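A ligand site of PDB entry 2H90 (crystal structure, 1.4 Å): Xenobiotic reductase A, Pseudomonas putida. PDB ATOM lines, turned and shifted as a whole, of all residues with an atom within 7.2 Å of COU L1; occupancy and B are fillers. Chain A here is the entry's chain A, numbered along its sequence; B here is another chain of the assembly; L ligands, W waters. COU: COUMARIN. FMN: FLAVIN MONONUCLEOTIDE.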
ATOM      1  N   PRO A  22      15.060 -25.341  -1.609  1.00  0.00           N
ATOM      2  CA  PRO A  22      15.711 -24.051  -1.856  1.00  0.00           C
ATOM      3  C   PRO A  22      15.283 -23.032  -0.812  1.00  0.00           C
ATOM      4  O   PRO A  22      14.111 -22.933  -0.478  1.00  0.00           O
ATOM      5  CB  PRO A  22      15.231 -23.696  -3.268  1.00  0.00           C
ATOM      6  CG  PRO A  22      13.909 -24.430  -3.397  1.00  0.00           C
ATOM      7  CD  PRO A  22      14.244 -25.750  -2.766  1.00  0.00           C
ATOM      8  N   MET A  23      16.259 -22.319  -0.258  1.00  0.00           N
ATOM      9  CA  MET A  23      15.973 -21.298   0.735  1.00  0.00           C
ATOM     10  C   MET A  23      16.826 -20.057   0.516  1.00  0.00           C
ATOM     11  O   MET A  23      18.026 -20.050   0.819  1.00  0.00           O
ATOM     12  CB  MET A  23      16.176 -21.829   2.157  1.00  0.00           C
ATOM     13  CG  MET A  23      15.096 -22.820   2.620  1.00  0.00           C
ATOM     14  SD  MET A  23      15.298 -23.293   4.356  1.00  0.00           S
ATOM     15  CE  MET A  23      16.666 -24.445   4.214  1.00  0.00           C
ATOM     16  N   CYS A  24      16.199 -19.021  -0.041  1.00  0.00           N
ATOM     17  CA  CYS A  24      16.870 -17.754  -0.309  1.00  0.00           C
ATOM     18  C   CYS A  24      17.573 -17.235   0.940  1.00  0.00           C
ATOM     19  O   CYS A  24      17.026 -17.282   2.050  1.00  0.00           O
ATOM     20  CB  CYS A  24      15.855 -16.706  -0.768  1.00  0.00           C
ATOM     21  SG  CYS A  24      15.310 -16.872  -2.476  1.00  0.00           S
ATOM     22  N   TYR A  26      19.333 -14.099   0.583  1.00  0.00           N
ATOM     23  CA  TYR A  26      19.338 -12.640   0.376  1.00  0.00           C
ATOM     24  C   TYR A  26      20.700 -12.038   0.734  1.00  0.00           C
ATOM     25  O   TYR A  26      20.785 -10.904   1.209  1.00  0.00           O
ATOM     26  CB  TYR A  26      18.249 -12.007   1.241  1.00  0.00           C
ATOM     27  CG  TYR A  26      16.886 -12.626   1.038  1.00  0.00           C
ATOM     28  CD1 TYR A  26      16.061 -12.235  -0.011  1.00  0.00           C
ATOM     29  CD2 TYR A  26      16.432 -13.618   1.901  1.00  0.00           C
ATOM     30  CE1 TYR A  26      14.819 -12.829  -0.215  1.00  0.00           C
ATOM     31  CE2 TYR A  26      15.187 -14.226   1.717  1.00  0.00           C
ATOM     32  CZ  TYR A  26      14.378 -13.815   0.649  1.00  0.00           C
ATOM     33  OH  TYR A  26      13.154 -14.402   0.467  1.00  0.00           O
ATOM     34  N   ALA A  56      16.583 -20.154  -4.833  1.00  0.00           N
ATOM     35  CA  ALA A  56      16.115 -19.609  -6.108  1.00  0.00           C
ATOM     36  C   ALA A  56      17.210 -18.719  -6.682  1.00  0.00           C
ATOM     37  O   ALA A  56      17.572 -17.689  -6.102  1.00  0.00           O
ATOM     38  CB  ALA A  56      14.838 -18.793  -5.879  1.00  0.00           C
ATOM     39  N   ILE A  65      14.284 -11.786  -6.903  1.00  0.00           N
ATOM     40  CA  ILE A  65      13.168 -11.353  -6.091  1.00  0.00           C
ATOM     41  C   ILE A  65      13.603 -10.036  -5.445  1.00  0.00           C
ATOM     42  O   ILE A  65      12.848  -9.055  -5.422  1.00  0.00           O
ATOM     43  CB  ILE A  65      12.861 -12.361  -4.953  1.00  0.00           C
ATOM     44  CG1 ILE A  65      12.523 -13.723  -5.541  1.00  0.00           C
ATOM     45  CG2 ILE A  65      11.701 -11.840  -4.096  1.00  0.00           C
ATOM     46  CD1 ILE A  65      12.523 -14.837  -4.509  1.00  0.00           C
ATOM     47  N   CYS A  69      19.336 -11.431  -4.030  1.00  0.00           N
ATOM     48  CA  CYS A  69      19.178 -12.763  -4.602  1.00  0.00           C
ATOM     49  C   CYS A  69      20.333 -13.220  -5.478  1.00  0.00           C
ATOM     50  O   CYS A  69      20.987 -12.426  -6.152  1.00  0.00           O
ATOM     51  CB  CYS A  69      17.884 -12.833  -5.422  1.00  0.00           C
ATOM     52  SG  CYS A  69      16.397 -12.803  -4.402  1.00  0.00           S
ATOM     53  N   GLN A  98      17.812 -24.458  -7.792  1.00  0.00           N
ATOM     54  CA  GLN A  98      16.527 -24.024  -8.304  1.00  0.00           C
ATOM     55  C   GLN A  98      16.776 -22.753  -9.127  1.00  0.00           C
ATOM     56  O   GLN A  98      17.266 -21.771  -8.594  1.00  0.00           O
ATOM     57  CB  GLN A  98      15.576 -23.688  -7.150  1.00  0.00           C
ATOM     58  CG  GLN A  98      14.198 -23.232  -7.608  1.00  0.00           C
ATOM     59  CD  GLN A  98      13.353 -22.702  -6.476  1.00  0.00           C
ATOM     60  OE1 GLN A  98      13.717 -21.717  -5.827  1.00  0.00           O
ATOM     61  NE2 GLN A  98      12.213 -23.338  -6.225  1.00  0.00           N
ATOM     62  N   PRO A 111      13.260  -9.689   3.165  1.00  0.00           N
ATOM     63  CA  PRO A 111      12.203  -9.886   4.156  1.00  0.00           C
ATOM     64  C   PRO A 111      12.352  -9.077   5.446  1.00  0.00           C
ATOM     65  O   PRO A 111      11.363  -8.599   6.004  1.00  0.00           O
ATOM     66  CB  PRO A 111      12.236 -11.395   4.391  1.00  0.00           C
ATOM     67  CG  PRO A 111      12.631 -11.922   3.035  1.00  0.00           C
ATOM     68  CD  PRO A 111      13.763 -10.987   2.671  1.00  0.00           C
ATOM     69  N   ASP A 115      10.216  -6.294   3.134  1.00  0.00           N
ATOM     70  CA  ASP A 115       9.575  -7.398   2.433  1.00  0.00           C
ATOM     71  C   ASP A 115       8.584  -6.918   1.368  1.00  0.00           C
ATOM     72  O   ASP A 115       7.843  -7.729   0.791  1.00  0.00           O
ATOM     73  CB  ASP A 115       8.850  -8.301   3.446  1.00  0.00           C
ATOM     74  CG  ASP A 115       8.473  -9.649   2.872  1.00  0.00           C
ATOM     75  OD1 ASP A 115       9.364 -10.317   2.316  1.00  0.00           O
ATOM     76  OD2 ASP A 115       7.291 -10.046   2.991  1.00  0.00           O
ATOM     77  N   HIS A 177      11.730 -23.251 -11.135  1.00  0.00           N
ATOM     78  CA  HIS A 177      10.816 -22.615 -10.199  1.00  0.00           C
ATOM     79  C   HIS A 177       9.528 -22.112 -10.829  1.00  0.00           C
ATOM     80  O   HIS A 177       9.417 -20.947 -11.210  1.00  0.00           O
ATOM     81  CB  HIS A 177      11.526 -21.457  -9.493  1.00  0.00           C
ATOM     82  CG  HIS A 177      10.877 -21.048  -8.210  1.00  0.00           C
ATOM     83  ND1 HIS A 177       9.634 -21.516  -7.828  1.00  0.00           N
ATOM     84  CD2 HIS A 177      11.298 -20.246  -7.207  1.00  0.00           C
ATOM     85  CE1 HIS A 177       9.330 -21.029  -6.641  1.00  0.00           C
ATOM     86  NE2 HIS A 177      10.321 -20.261  -6.240  1.00  0.00           N
ATOM     87  N   ALA A 179       6.637 -22.123  -9.207  1.00  0.00           N
ATOM     88  CA  ALA A 179       5.691 -21.971  -8.111  1.00  0.00           C
ATOM     89  C   ALA A 179       5.789 -20.627  -7.414  1.00  0.00           C
ATOM     90  O   ALA A 179       6.532 -19.743  -7.817  1.00  0.00           O
ATOM     91  CB  ALA A 179       5.908 -23.093  -7.093  1.00  0.00           C
ATOM     92  N   HIS A 180       4.985 -20.507  -6.356  1.00  0.00           N
ATOM     93  CA  HIS A 180       4.952 -19.341  -5.488  1.00  0.00           C
ATOM     94  C   HIS A 180       4.631 -17.970  -6.080  1.00  0.00           C
ATOM     95  O   HIS A 180       5.060 -16.940  -5.569  1.00  0.00           O
ATOM     96  CB  HIS A 180       6.274 -19.323  -4.698  1.00  0.00           C
ATOM     97  CG  HIS A 180       6.513 -20.593  -3.926  1.00  0.00           C
ATOM     98  ND1 HIS A 180       7.716 -20.881  -3.319  1.00  0.00           N
ATOM     99  CD2 HIS A 180       5.693 -21.643  -3.668  1.00  0.00           C
ATOM    100  CE1 HIS A 180       7.631 -22.057  -2.718  1.00  0.00           C
ATOM    101  NE2 HIS A 180       6.415 -22.539  -2.917  1.00  0.00           N
ATOM    102  N   GLY A 181       3.854 -17.976  -7.160  1.00  0.00           N
ATOM    103  CA  GLY A 181       3.424 -16.735  -7.777  1.00  0.00           C
ATOM    104  C   GLY A 181       4.423 -16.004  -8.631  1.00  0.00           C
ATOM    105  O   GLY A 181       4.161 -14.876  -9.078  1.00  0.00           O
ATOM    106  N   TYR A 182       5.573 -16.615  -8.870  1.00  0.00           N
ATOM    107  CA  TYR A 182       6.590 -15.976  -9.692  1.00  0.00           C
ATOM    108  C   TYR A 182       6.226 -16.140 -11.160  1.00  0.00           C
ATOM    109  O   TYR A 182       5.117 -16.569 -11.479  1.00  0.00           O
ATOM    110  CB  TYR A 182       7.973 -16.559  -9.353  1.00  0.00           C
ATOM    111  CG  TYR A 182       8.353 -16.309  -7.903  1.00  0.00           C
ATOM    112  CD1 TYR A 182       8.346 -15.021  -7.368  1.00  0.00           C
ATOM    113  CD2 TYR A 182       8.672 -17.377  -7.055  1.00  0.00           C
ATOM    114  CE1 TYR A 182       8.659 -14.799  -6.027  1.00  0.00           C
ATOM    115  CE2 TYR A 182       8.986 -17.155  -5.714  1.00  0.00           C
ATOM    116  CZ  TYR A 182       8.973 -15.870  -5.201  1.00  0.00           C
ATOM    117  OH  TYR A 182       9.258 -15.650  -3.876  1.00  0.00           O
ATOM    118  N   ARG A 230       9.304 -27.088  -9.322  1.00  0.00           N
ATOM    119  CA  ARG A 230       8.451 -26.827  -8.167  1.00  0.00           C
ATOM    120  C   ARG A 230       7.240 -26.156  -8.785  1.00  0.00           C
ATOM    121  O   ARG A 230       7.378 -25.290  -9.653  1.00  0.00           O
ATOM    122  CB  ARG A 230       9.135 -25.923  -7.134  1.00  0.00           C
ATOM    123  CG  ARG A 230       8.410 -25.940  -5.796  1.00  0.00           C
ATOM    124  CD  ARG A 230       9.227 -25.364  -4.646  1.00  0.00           C
ATOM    125  NE  ARG A 230       8.819 -25.991  -3.388  1.00  0.00           N
ATOM    126  CZ  ARG A 230       9.296 -25.666  -2.192  1.00  0.00           C
ATOM    127  NH1 ARG A 230      10.195 -24.701  -2.068  1.00  0.00           N
ATOM    128  NH2 ARG A 230       8.913 -26.354  -1.120  1.00  0.00           N
ATOM    129  N   PHE A 268       0.426 -19.209  -4.229  1.00  0.00           N
ATOM    130  CA  PHE A 268       0.785 -17.879  -3.727  1.00  0.00           C
ATOM    131  C   PHE A 268       0.718 -16.860  -4.858  1.00  0.00           C
ATOM    132  O   PHE A 268       1.491 -15.906  -4.896  1.00  0.00           O
ATOM    133  CB  PHE A 268       2.198 -17.879  -3.140  1.00  0.00           C
ATOM    134  CG  PHE A 268       2.351 -18.727  -1.927  1.00  0.00           C
ATOM    135  CD1 PHE A 268       1.643 -18.442  -0.766  1.00  0.00           C
ATOM    136  CD2 PHE A 268       3.204 -19.816  -1.952  1.00  0.00           C
ATOM    137  CE1 PHE A 268       1.785 -19.237   0.357  1.00  0.00           C
ATOM    138  CE2 PHE A 268       3.350 -20.620  -0.829  1.00  0.00           C
ATOM    139  CZ  PHE A 268       2.638 -20.326   0.333  1.00  0.00           C
ATOM    140  N   TRP A 301       6.832 -28.111   4.546  1.00  0.00           N
ATOM    141  CA  TRP A 301       6.117 -27.361   5.573  1.00  0.00           C
ATOM    142  C   TRP A 301       5.781 -28.186   6.803  1.00  0.00           C
ATOM    143  O   TRP A 301       4.807 -28.947   6.828  1.00  0.00           O
ATOM    144  CB  TRP A 301       4.842 -26.700   5.051  1.00  0.00           C
ATOM    145  CG  TRP A 301       4.296 -25.725   6.060  1.00  0.00           C
ATOM    146  CD1 TRP A 301       3.569 -26.024   7.179  1.00  0.00           C
ATOM    147  CD2 TRP A 301       4.532 -24.308   6.107  1.00  0.00           C
ATOM    148  NE1 TRP A 301       3.353 -24.885   7.925  1.00  0.00           N
ATOM    149  CE2 TRP A 301       3.936 -23.816   7.290  1.00  0.00           C
ATOM    150  CE3 TRP A 301       5.198 -23.403   5.262  1.00  0.00           C
ATOM    151  CZ2 TRP A 301       3.985 -22.474   7.653  1.00  0.00           C
ATOM    152  CZ3 TRP A 301       5.247 -22.062   5.625  1.00  0.00           C
ATOM    153  CH2 TRP A 301       4.645 -21.606   6.813  1.00  0.00           C
ATOM    154  N   HIS B 356      15.462 -14.271  11.063  1.00  0.00           N
ATOM    155  CA  HIS B 356      14.187 -13.734  10.613  1.00  0.00           C
ATOM    156  C   HIS B 356      13.093 -14.793  10.548  1.00  0.00           C
ATOM    157  O   HIS B 356      11.945 -14.528  10.884  1.00  0.00           O
ATOM    158  CB  HIS B 356      14.354 -13.096   9.240  1.00  0.00           C
ATOM    159  CG  HIS B 356      13.108 -12.432   8.733  1.00  0.00           C
ATOM    160  ND1 HIS B 356      12.668 -11.216   9.219  1.00  0.00           N
ATOM    161  CD2 HIS B 356      12.200 -12.826   7.807  1.00  0.00           C
ATOM    162  CE1 HIS B 356      11.535 -10.894   8.609  1.00  0.00           C
ATOM    163  NE2 HIS B 356      11.230 -11.845   7.752  1.00  0.00           N
ATOM    164  N   TRP B 357      13.467 -16.011  10.145  1.00  0.00           N
ATOM    165  CA  TRP B 357      12.501 -17.096   9.985  1.00  0.00           C
ATOM    166  C   TRP B 357      12.271 -17.992  11.180  1.00  0.00           C
ATOM    167  O   TRP B 357      11.363 -18.820  11.162  1.00  0.00           O
ATOM    168  CB  TRP B 357      12.932 -17.954   8.799  1.00  0.00           C
ATOM    169  CG  TRP B 357      13.386 -17.108   7.667  1.00  0.00           C
ATOM    170  CD1 TRP B 357      14.680 -16.774   7.372  1.00  0.00           C
ATOM    171  CD2 TRP B 357      12.564 -16.409   6.746  1.00  0.00           C
ATOM    172  NE1 TRP B 357      14.706 -15.880   6.317  1.00  0.00           N
ATOM    173  CE2 TRP B 357      13.411 -15.641   5.923  1.00  0.00           C
ATOM    174  CE3 TRP B 357      11.181 -16.340   6.539  1.00  0.00           C
ATOM    175  CZ2 TRP B 357      12.931 -14.821   4.894  1.00  0.00           C
ATOM    176  CZ3 TRP B 357      10.693 -15.524   5.531  1.00  0.00           C
ATOM    177  CH2 TRP B 357      11.572 -14.774   4.715  1.00  0.00           C
HETATM  178  C1  COU L   1      10.172 -18.520  -2.558  1.00  0.00           C
HETATM  179  C2  COU L   1      11.288 -17.485  -2.423  1.00  0.00           C
HETATM  180  C3  COU L   1      11.534 -16.881  -1.258  1.00  0.00           C
HETATM  181  C4  COU L   1      10.725 -17.200  -0.051  1.00  0.00           C
HETATM  182  C5  COU L   1      10.932 -16.595   1.225  1.00  0.00           C
HETATM  183  C6  COU L   1      10.122 -16.944   2.310  1.00  0.00           C
HETATM  184  C7  COU L   1       9.083 -17.908   2.153  1.00  0.00           C
HETATM  185  C8  COU L   1       8.861 -18.521   0.918  1.00  0.00           C
HETATM  186  C9  COU L   1       9.673 -18.170  -0.195  1.00  0.00           C
HETATM  187  O1  COU L   1       9.893 -19.122  -3.575  1.00  0.00           O
HETATM  188  O2  COU L   1       9.404 -18.818  -1.405  1.00  0.00           O
HETATM  189  N1  FMN L   2      10.915 -21.964  -1.805  1.00  0.00           N
HETATM  190  C2  FMN L   2      11.290 -21.971  -3.130  1.00  0.00           C
HETATM  191  O2  FMN L   2      10.707 -22.557  -3.917  1.00  0.00           O
HETATM  192  N3  FMN L   2      12.537 -21.170  -3.461  1.00  0.00           N
HETATM  193  C4  FMN L   2      13.322 -20.415  -2.537  1.00  0.00           C
HETATM  194  O4  FMN L   2      14.326 -19.796  -2.858  1.00  0.00           O
HETATM  195  C4A FMN L   2      12.872 -20.424  -1.131  1.00  0.00           C
HETATM  196  N5  FMN L   2      13.556 -19.729  -0.158  1.00  0.00           N
HETATM  197  C5A FMN L   2      13.168 -19.730   1.194  1.00  0.00           C
HETATM  198  C6  FMN L   2      14.028 -18.939   2.137  1.00  0.00           C
HETATM  199  C7  FMN L   2      13.660 -18.953   3.517  1.00  0.00           C
HETATM  200  C7M FMN L   2      14.557 -18.185   4.304  1.00  0.00           C
HETATM  201  C8  FMN L   2      12.368 -19.760   4.101  1.00  0.00           C
HETATM  202  C8M FMN L   2      11.918 -19.855   5.404  1.00  0.00           C
HETATM  203  C9  FMN L   2      11.648 -20.451   3.155  1.00  0.00           C
HETATM  204  C9A FMN L   2      11.954 -20.507   1.677  1.00  0.00           C
HETATM  205  N10 FMN L   2      11.210 -21.271   0.535  1.00  0.00           N
HETATM  206  C10 FMN L   2      11.600 -21.268  -0.846  1.00  0.00           C
HETATM  207  C1' FMN L   2      10.053 -22.032   1.006  1.00  0.00           C
HETATM  208  C2' FMN L   2      10.864 -23.400   1.519  1.00  0.00           C
HETATM  209  O2' FMN L   2      11.539 -24.123   0.435  1.00  0.00           O
HETATM  210  C3' FMN L   2       9.991 -24.452   2.143  1.00  0.00           C
HETATM  211  O3' FMN L   2       9.055 -25.002   1.202  1.00  0.00           O
HETATM  212  C4' FMN L   2       9.226 -23.819   3.347  1.00  0.00           C
HETATM  213  O4' FMN L   2      10.121 -23.223   4.332  1.00  0.00           O
HETATM  214  C5' FMN L   2       8.366 -24.845   4.058  1.00  0.00           C
HETATM  215  O5' FMN L   2       9.240 -25.922   4.737  1.00  0.00           O
HETATM  216  P   FMN L   2       9.687 -25.842   6.274  1.00  0.00           P
HETATM  217  O1P FMN L   2      10.506 -24.652   6.490  1.00  0.00           O
HETATM  218  O2P FMN L   2       8.439 -25.817   7.140  1.00  0.00           O
HETATM  219  O3P FMN L   2      10.517 -27.126   6.459  1.00  0.00           O
HETATM  220  O   HOH W   1       6.629 -20.714  -0.059  1.00  0.00           O
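A ring nitrogen (ND1) of His 177 sits close to the backbone NH of Ala 179 (3.4 Å).
The side-chain sulfur (SG) of Cys 69 sits at hydrogen-bond distance from the backbone NH (N) of Ile 65 (3.4 Å).
NE2 of His 177 is in hydrogen-bond range of O2 of FMN L2 (3.3 Å).
The side-chain amide oxygen (OE1) of Gln 98 lies within hydrogen-bond range of a nitrogen (N3) of FMN L2 (2.7 Å).
N of Ala 56 sits at hydrogen-bond distance from O4 of FMN L2 (3.0 Å).
The backbone NH (N) of Cys 24 sits at hydrogen-bond distance from a nitrogen (N5) of FMN L2, at 2.7 Å.
An oxygen (O1) of COU L1 lies within hydrogen-bond range of a ring nitrogen (NE2) of His 177 (2.9 Å).
O2 of FMN L2 sits close to ND1 of His 180 (3.5 Å).
The backbone carbonyl oxygen of Pro 22 sits close to an oxygen (O2') of FMN L2.
N of Trp 301 lies within hydrogen-bond range of O5' of FMN L2 (3.3 Å).
NH2 of Arg 230 sits at hydrogen-bond distance from O3' of FMN L2 (2.7 Å).
O1 of COU L1 lies within hydrogen-bond range of ND1 of His 180, at 2.8 Å.
The side-chain sulfur of Cys 24 lies within hydrogen-bond range of an oxygen (O4) of FMN L2.
An oxygen (O1) of COU L1 sits close to a nitrogen (N3) of FMN L2, 3.3 Å away.
SG of Cys 24 touches C3 of COU L1, 3.97 Å away.
OH of Tyr 26 touches C5 of COU L1, at 3.2 Å.
CD1 of Ile 65 touches C2 of COU L1 (3.6 Å).
CE2 of Tyr 182 touches O1 of COU L1, at 3.0 Å.
CH2 of Trp 357 of chain B touches C6 of COU L1, 3.5 Å away.
Hydrophobic or aromatic side chains within 4 Å of COU L1: Ile 65, His 177, His 180, Tyr 182 and Trp 357 of chain B.
Of the 20 residues printed, 7 come within 4 Å of COU L1.
The nearest printed residue that does not touch COU L1 is Ala 56 (5.1 Å).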
